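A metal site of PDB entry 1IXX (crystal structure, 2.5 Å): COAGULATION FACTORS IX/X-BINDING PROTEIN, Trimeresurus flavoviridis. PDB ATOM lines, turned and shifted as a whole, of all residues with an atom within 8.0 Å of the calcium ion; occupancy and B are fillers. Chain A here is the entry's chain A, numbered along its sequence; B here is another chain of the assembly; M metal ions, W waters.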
ATOM      1  N   TYR A   9     -22.390  27.947  -9.967  1.00  0.00           N
ATOM      2  CA  TYR A   9     -22.208  26.530  -9.647  1.00  0.00           C
ATOM      3  C   TYR A   9     -21.080  26.408  -8.660  1.00  0.00           C
ATOM      4  O   TYR A   9     -19.926  26.703  -8.984  1.00  0.00           O
ATOM      5  CB  TYR A   9     -21.886  25.719 -10.887  1.00  0.00           C
ATOM      6  CG  TYR A   9     -21.526  24.280 -10.562  1.00  0.00           C
ATOM      7  CD1 TYR A   9     -22.447  23.441  -9.934  1.00  0.00           C
ATOM      8  CD2 TYR A   9     -20.265  23.758 -10.872  1.00  0.00           C
ATOM      9  CE1 TYR A   9     -22.130  22.129  -9.624  1.00  0.00           C
ATOM     10  CE2 TYR A   9     -19.948  22.457 -10.562  1.00  0.00           C
ATOM     11  CZ  TYR A   9     -20.881  21.647  -9.938  1.00  0.00           C
ATOM     12  OH  TYR A   9     -20.589  20.334  -9.647  1.00  0.00           O
ATOM     13  N   GLU A  10     -21.411  26.007  -7.448  1.00  0.00           N
ATOM     14  CA  GLU A  10     -20.417  25.841  -6.398  1.00  0.00           C
ATOM     15  C   GLU A  10     -19.566  27.090  -6.151  1.00  0.00           C
ATOM     16  O   GLU A  10     -18.338  27.016  -6.131  1.00  0.00           O
ATOM     17  CB  GLU A  10     -19.530  24.635  -6.694  1.00  0.00           C
ATOM     18  CG  GLU A  10     -20.272  23.308  -6.621  1.00  0.00           C
ATOM     19  CD  GLU A  10     -19.377  22.094  -6.840  1.00  0.00           C
ATOM     20  OE1 GLU A  10     -18.188  22.270  -7.193  1.00  0.00           O
ATOM     21  OE2 GLU A  10     -19.862  20.960  -6.645  1.00  0.00           O
ATOM     22  N   HIS A  12     -19.073  29.962  -8.049  1.00  0.00           N
ATOM     23  CA  HIS A  12     -18.357  30.500  -9.202  1.00  0.00           C
ATOM     24  C   HIS A  12     -19.409  30.783 -10.251  1.00  0.00           C
ATOM     25  O   HIS A  12     -20.511  30.224 -10.179  1.00  0.00           O
ATOM     26  CB  HIS A  12     -17.363  29.491  -9.760  1.00  0.00           C
ATOM     27  CG  HIS A  12     -16.058  29.469  -9.043  1.00  0.00           C
ATOM     28  ND1 HIS A  12     -15.292  30.603  -8.873  1.00  0.00           N
ATOM     29  CD2 HIS A  12     -15.389  28.468  -8.434  1.00  0.00           C
ATOM     30  CE1 HIS A  12     -14.207  30.301  -8.182  1.00  0.00           C
ATOM     31  NE2 HIS A  12     -14.248  29.005  -7.904  1.00  0.00           N
ATOM     32  N   CYS A  13     -19.066  31.602 -11.234  1.00  0.00           N
ATOM     33  CA  CYS A  13     -19.991  31.960 -12.295  1.00  0.00           C
ATOM     34  C   CYS A  13     -19.494  31.523 -13.642  1.00  0.00           C
ATOM     35  O   CYS A  13     -18.331  31.718 -13.983  1.00  0.00           O
ATOM     36  CB  CYS A  13     -20.209  33.463 -12.292  1.00  0.00           C
ATOM     37  SG  CYS A  13     -20.871  34.070 -10.717  1.00  0.00           S
ATOM     38  N   TYR A  14     -20.401  30.948 -14.432  1.00  0.00           N
ATOM     39  CA  TYR A  14     -20.067  30.456 -15.757  1.00  0.00           C
ATOM     40  C   TYR A  14     -20.939  31.085 -16.857  1.00  0.00           C
ATOM     41  O   TYR A  14     -22.060  31.510 -16.606  1.00  0.00           O
ATOM     42  CB  TYR A  14     -20.235  28.928 -15.769  1.00  0.00           C
ATOM     43  CG  TYR A  14     -19.441  28.194 -14.703  1.00  0.00           C
ATOM     44  CD1 TYR A  14     -19.921  28.080 -13.396  1.00  0.00           C
ATOM     45  CD2 TYR A  14     -18.231  27.581 -15.007  1.00  0.00           C
ATOM     46  CE1 TYR A  14     -19.203  27.391 -12.428  1.00  0.00           C
ATOM     47  CE2 TYR A  14     -17.510  26.892 -14.049  1.00  0.00           C
ATOM     48  CZ  TYR A  14     -18.007  26.797 -12.758  1.00  0.00           C
ATOM     49  OH  TYR A  14     -17.248  26.129 -11.820  1.00  0.00           O
ATOM     50  N   LEU A  39     -10.972  31.422 -19.007  1.00  0.00           N
ATOM     51  CA  LEU A  39     -11.693  30.317 -19.646  1.00  0.00           C
ATOM     52  C   LEU A  39     -11.955  29.294 -18.560  1.00  0.00           C
ATOM     53  O   LEU A  39     -11.172  29.158 -17.611  1.00  0.00           O
ATOM     54  CB  LEU A  39     -10.864  29.699 -20.757  1.00  0.00           C
ATOM     55  CG  LEU A  39     -10.980  30.420 -22.097  1.00  0.00           C
ATOM     56  CD1 LEU A  39     -10.027  29.809 -23.104  1.00  0.00           C
ATOM     57  CD2 LEU A  39     -12.421  30.323 -22.604  1.00  0.00           C
ATOM     58  N   VAL A  40     -13.024  28.539 -18.727  1.00  0.00           N
ATOM     59  CA  VAL A  40     -13.401  27.540 -17.743  1.00  0.00           C
ATOM     60  C   VAL A  40     -12.319  26.519 -17.367  1.00  0.00           C
ATOM     61  O   VAL A  40     -11.568  26.024 -18.221  1.00  0.00           O
ATOM     62  CB  VAL A  40     -14.698  26.820 -18.152  1.00  0.00           C
ATOM     63  CG1 VAL A  40     -14.477  25.995 -19.404  1.00  0.00           C
ATOM     64  CG2 VAL A  40     -15.242  25.989 -17.003  1.00  0.00           C
ATOM     65  N   SER A  41     -12.175  26.308 -16.057  1.00  0.00           N
ATOM     66  CA  SER A  41     -11.238  25.337 -15.498  1.00  0.00           C
ATOM     67  C   SER A  41     -12.107  24.280 -14.840  1.00  0.00           C
ATOM     68  O   SER A  41     -12.801  24.561 -13.838  1.00  0.00           O
ATOM     69  CB  SER A  41     -10.328  25.979 -14.434  1.00  0.00           C
ATOM     70  OG  SER A  41     -11.070  26.391 -13.303  1.00  0.00           O
ATOM     71  N   ILE A  42     -12.119  23.093 -15.447  1.00  0.00           N
ATOM     72  CA  ILE A  42     -12.893  21.965 -14.978  1.00  0.00           C
ATOM     73  C   ILE A  42     -12.041  21.182 -13.987  1.00  0.00           C
ATOM     74  O   ILE A  42     -11.036  20.599 -14.347  1.00  0.00           O
ATOM     75  CB  ILE A  42     -13.324  21.077 -16.156  1.00  0.00           C
ATOM     76  CG1 ILE A  42     -14.156  21.932 -17.121  1.00  0.00           C
ATOM     77  CG2 ILE A  42     -14.123  19.879 -15.662  1.00  0.00           C
ATOM     78  CD1 ILE A  42     -14.542  21.274 -18.403  1.00  0.00           C
ATOM     79  N   GLU A  43     -12.451  21.219 -12.722  1.00  0.00           N
ATOM     80  CA  GLU A  43     -11.711  20.563 -11.664  1.00  0.00           C
ATOM     81  C   GLU A  43     -12.398  19.363 -11.029  1.00  0.00           C
ATOM     82  O   GLU A  43     -11.864  18.767 -10.091  1.00  0.00           O
ATOM     83  CB  GLU A  43     -11.357  21.595 -10.597  1.00  0.00           C
ATOM     84  CG  GLU A  43     -10.246  22.506 -11.038  1.00  0.00           C
ATOM     85  CD  GLU A  43     -10.407  23.906 -10.510  1.00  0.00           C
ATOM     86  OE1 GLU A  43      -9.916  24.193  -9.399  1.00  0.00           O
ATOM     87  OE2 GLU A  43     -11.001  24.726 -11.229  1.00  0.00           O
ATOM     88  N   SER A  44     -13.547  18.986 -11.553  1.00  0.00           N
ATOM     89  CA  SER A  44     -14.288  17.861 -11.021  1.00  0.00           C
ATOM     90  C   SER A  44     -15.336  17.356 -12.004  1.00  0.00           C
ATOM     91  O   SER A  44     -15.834  18.106 -12.849  1.00  0.00           O
ATOM     92  CB  SER A  44     -14.945  18.252  -9.694  1.00  0.00           C
ATOM     93  OG  SER A  44     -15.768  19.398  -9.850  1.00  0.00           O
ATOM     94  N   GLU A  47     -18.335  19.342 -12.183  1.00  0.00           N
ATOM     95  CA  GLU A  47     -18.135  20.581 -12.913  1.00  0.00           C
ATOM     96  C   GLU A  47     -18.149  20.242 -14.385  1.00  0.00           C
ATOM     97  O   GLU A  47     -18.639  21.024 -15.195  1.00  0.00           O
ATOM     98  CB  GLU A  47     -16.816  21.211 -12.527  1.00  0.00           C
ATOM     99  CG  GLU A  47     -16.700  22.646 -12.961  1.00  0.00           C
ATOM    100  CD  GLU A  47     -15.530  23.357 -12.319  1.00  0.00           C
ATOM    101  OE1 GLU A  47     -14.928  22.803 -11.370  1.00  0.00           O
ATOM    102  OE2 GLU A  47     -15.235  24.487 -12.775  1.00  0.00           O
ATOM    103  N   VAL A  51     -20.752  22.134 -16.820  1.00  0.00           N
ATOM    104  CA  VAL A  51     -20.337  22.829 -18.041  1.00  0.00           C
ATOM    105  C   VAL A  51     -20.961  22.193 -19.274  1.00  0.00           C
ATOM    106  O   VAL A  51     -21.426  22.892 -20.181  1.00  0.00           O
ATOM    107  CB  VAL A  51     -18.785  22.853 -18.159  1.00  0.00           C
ATOM    108  CG1 VAL A  51     -18.359  23.465 -19.501  1.00  0.00           C
ATOM    109  CG2 VAL A  51     -18.186  23.637 -16.998  1.00  0.00           C
ATOM    110  N   GLU A 128     -15.333  31.567 -16.763  1.00  0.00           N
ATOM    111  CA  GLU A 128     -15.581  31.284 -15.368  1.00  0.00           C
ATOM    112  C   GLU A 128     -15.008  32.418 -14.536  1.00  0.00           C
ATOM    113  O   GLU A 128     -13.925  32.941 -14.834  1.00  0.00           O
ATOM    114  CB  GLU A 128     -14.911  29.979 -14.944  1.00  0.00           C
ATOM    115  CG  GLU A 128     -15.199  29.655 -13.487  1.00  0.00           C
ATOM    116  CD  GLU A 128     -14.447  28.456 -12.975  1.00  0.00           C
ATOM    117  OE1 GLU A 128     -14.030  27.599 -13.784  1.00  0.00           O
ATOM    118  OE2 GLU A 128     -14.287  28.384 -11.734  1.00  0.00           O
ATOM    119  N   ALA A 129     -15.772  32.816 -13.527  1.00  0.00           N
ATOM    120  CA  ALA A 129     -15.382  33.866 -12.606  1.00  0.00           C
ATOM    121  C   ALA A 129     -15.565  33.275 -11.206  1.00  0.00           C
ATOM    122  O   ALA A 129     -14.576  32.786 -10.648  1.00  0.00           O
ATOM    123  CB  ALA A 129     -16.258  35.089 -12.801  1.00  0.00           C
ATOM    124  OXT ALA A 129     -16.717  33.224 -10.727  1.00  0.00           O
ATOM    125  N   TRP B  79      -3.779  25.648 -16.557  1.00  0.00           N
ATOM    126  CA  TRP B  79      -5.101  26.216 -16.678  1.00  0.00           C
ATOM    127  C   TRP B  79      -4.808  27.710 -16.624  1.00  0.00           C
ATOM    128  O   TRP B  79      -4.022  28.142 -15.766  1.00  0.00           O
ATOM    129  CB  TRP B  79      -5.959  25.835 -15.468  1.00  0.00           C
ATOM    130  CG  TRP B  79      -6.511  24.432 -15.480  1.00  0.00           C
ATOM    131  CD1 TRP B  79      -6.165  23.406 -14.649  1.00  0.00           C
ATOM    132  CD2 TRP B  79      -7.567  23.941 -16.309  1.00  0.00           C
ATOM    133  NE1 TRP B  79      -6.959  22.309 -14.901  1.00  0.00           N
ATOM    134  CE2 TRP B  79      -7.821  22.610 -15.921  1.00  0.00           C
ATOM    135  CE3 TRP B  79      -8.322  24.497 -17.339  1.00  0.00           C
ATOM    136  CZ2 TRP B  79      -8.795  21.827 -16.540  1.00  0.00           C
ATOM    137  CZ3 TRP B  79      -9.300  23.724 -17.949  1.00  0.00           C
ATOM    138  CH2 TRP B  79      -9.525  22.394 -17.552  1.00  0.00           C
ATOM    139  N   ASN B  81      -6.167  29.977 -15.246  1.00  0.00           N
ATOM    140  CA  ASN B  81      -6.483  30.540 -13.926  1.00  0.00           C
ATOM    141  C   ASN B  81      -5.540  29.983 -12.856  1.00  0.00           C
ATOM    142  O   ASN B  81      -5.735  30.236 -11.672  1.00  0.00           O
ATOM    143  CB  ASN B  81      -7.937  30.255 -13.552  1.00  0.00           C
ATOM    144  CG  ASN B  81      -8.177  28.815 -13.158  1.00  0.00           C
ATOM    145  OD1 ASN B  81      -8.936  28.531 -12.233  1.00  0.00           O
ATOM    146  ND2 ASN B  81      -7.573  27.878 -13.885  1.00  0.00           N
ATOM    147  N   ALA B  83      -5.234  26.926 -11.874  1.00  0.00           N
ATOM    148  CA  ALA B  83      -5.887  25.892 -11.072  1.00  0.00           C
ATOM    149  C   ALA B  83      -4.991  24.664 -11.070  1.00  0.00           C
ATOM    150  O   ALA B  83      -4.244  24.437 -12.013  1.00  0.00           O
ATOM    151  CB  ALA B  83      -7.235  25.545 -11.672  1.00  0.00           C
HETATM  152 CA    CA M   1     -13.281  25.985 -11.869  1.00  0.00          CA
HETATM  153  O   HOH W   1     -11.594  27.678 -10.789  1.00  0.00           O
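The calcium ion is bound by the backbone carbonyl oxygen (O) of Ser 41 (2.5 Å), the side-chain carboxylate (OE2) of Glu 128 (2.6 Å), the side-chain carboxylate (OE1) of Glu 128 (2.6 Å), the side-chain carboxylate (OE2) of Glu 47 (2.6 Å), water W1 (2.6 Å), the side-chain hydroxyl (OG) of Ser 41 (2.7 Å) and the side-chain carboxylate (OE2) of Glu 43 (2.7 Å). The calcium ion has seven donor atoms within binding distance.
Residues that only touch the calcium ion: Tyr 14 (3.97 Å). Of the 18 residues printed, 5 come within 4 Å of the calcium ion. The nearest printed residue that does not touch the calcium ion is His 12 (4.7 Å).
The side-chain hydroxyl (OG) of Ser 41 sits close to the side-chain amide oxygen (OD1) of Asn 81 of chain B, at 3.2 Å. The side-chain carboxylate (OE2) of Glu 47 sits close to the side-chain hydroxyl (OH) of Tyr 14, 2.8 Å away. The side-chain hydroxyl (OG) of Ser 44 sits close to the backbone NH (N) of Glu 47, 3.5 Å away.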
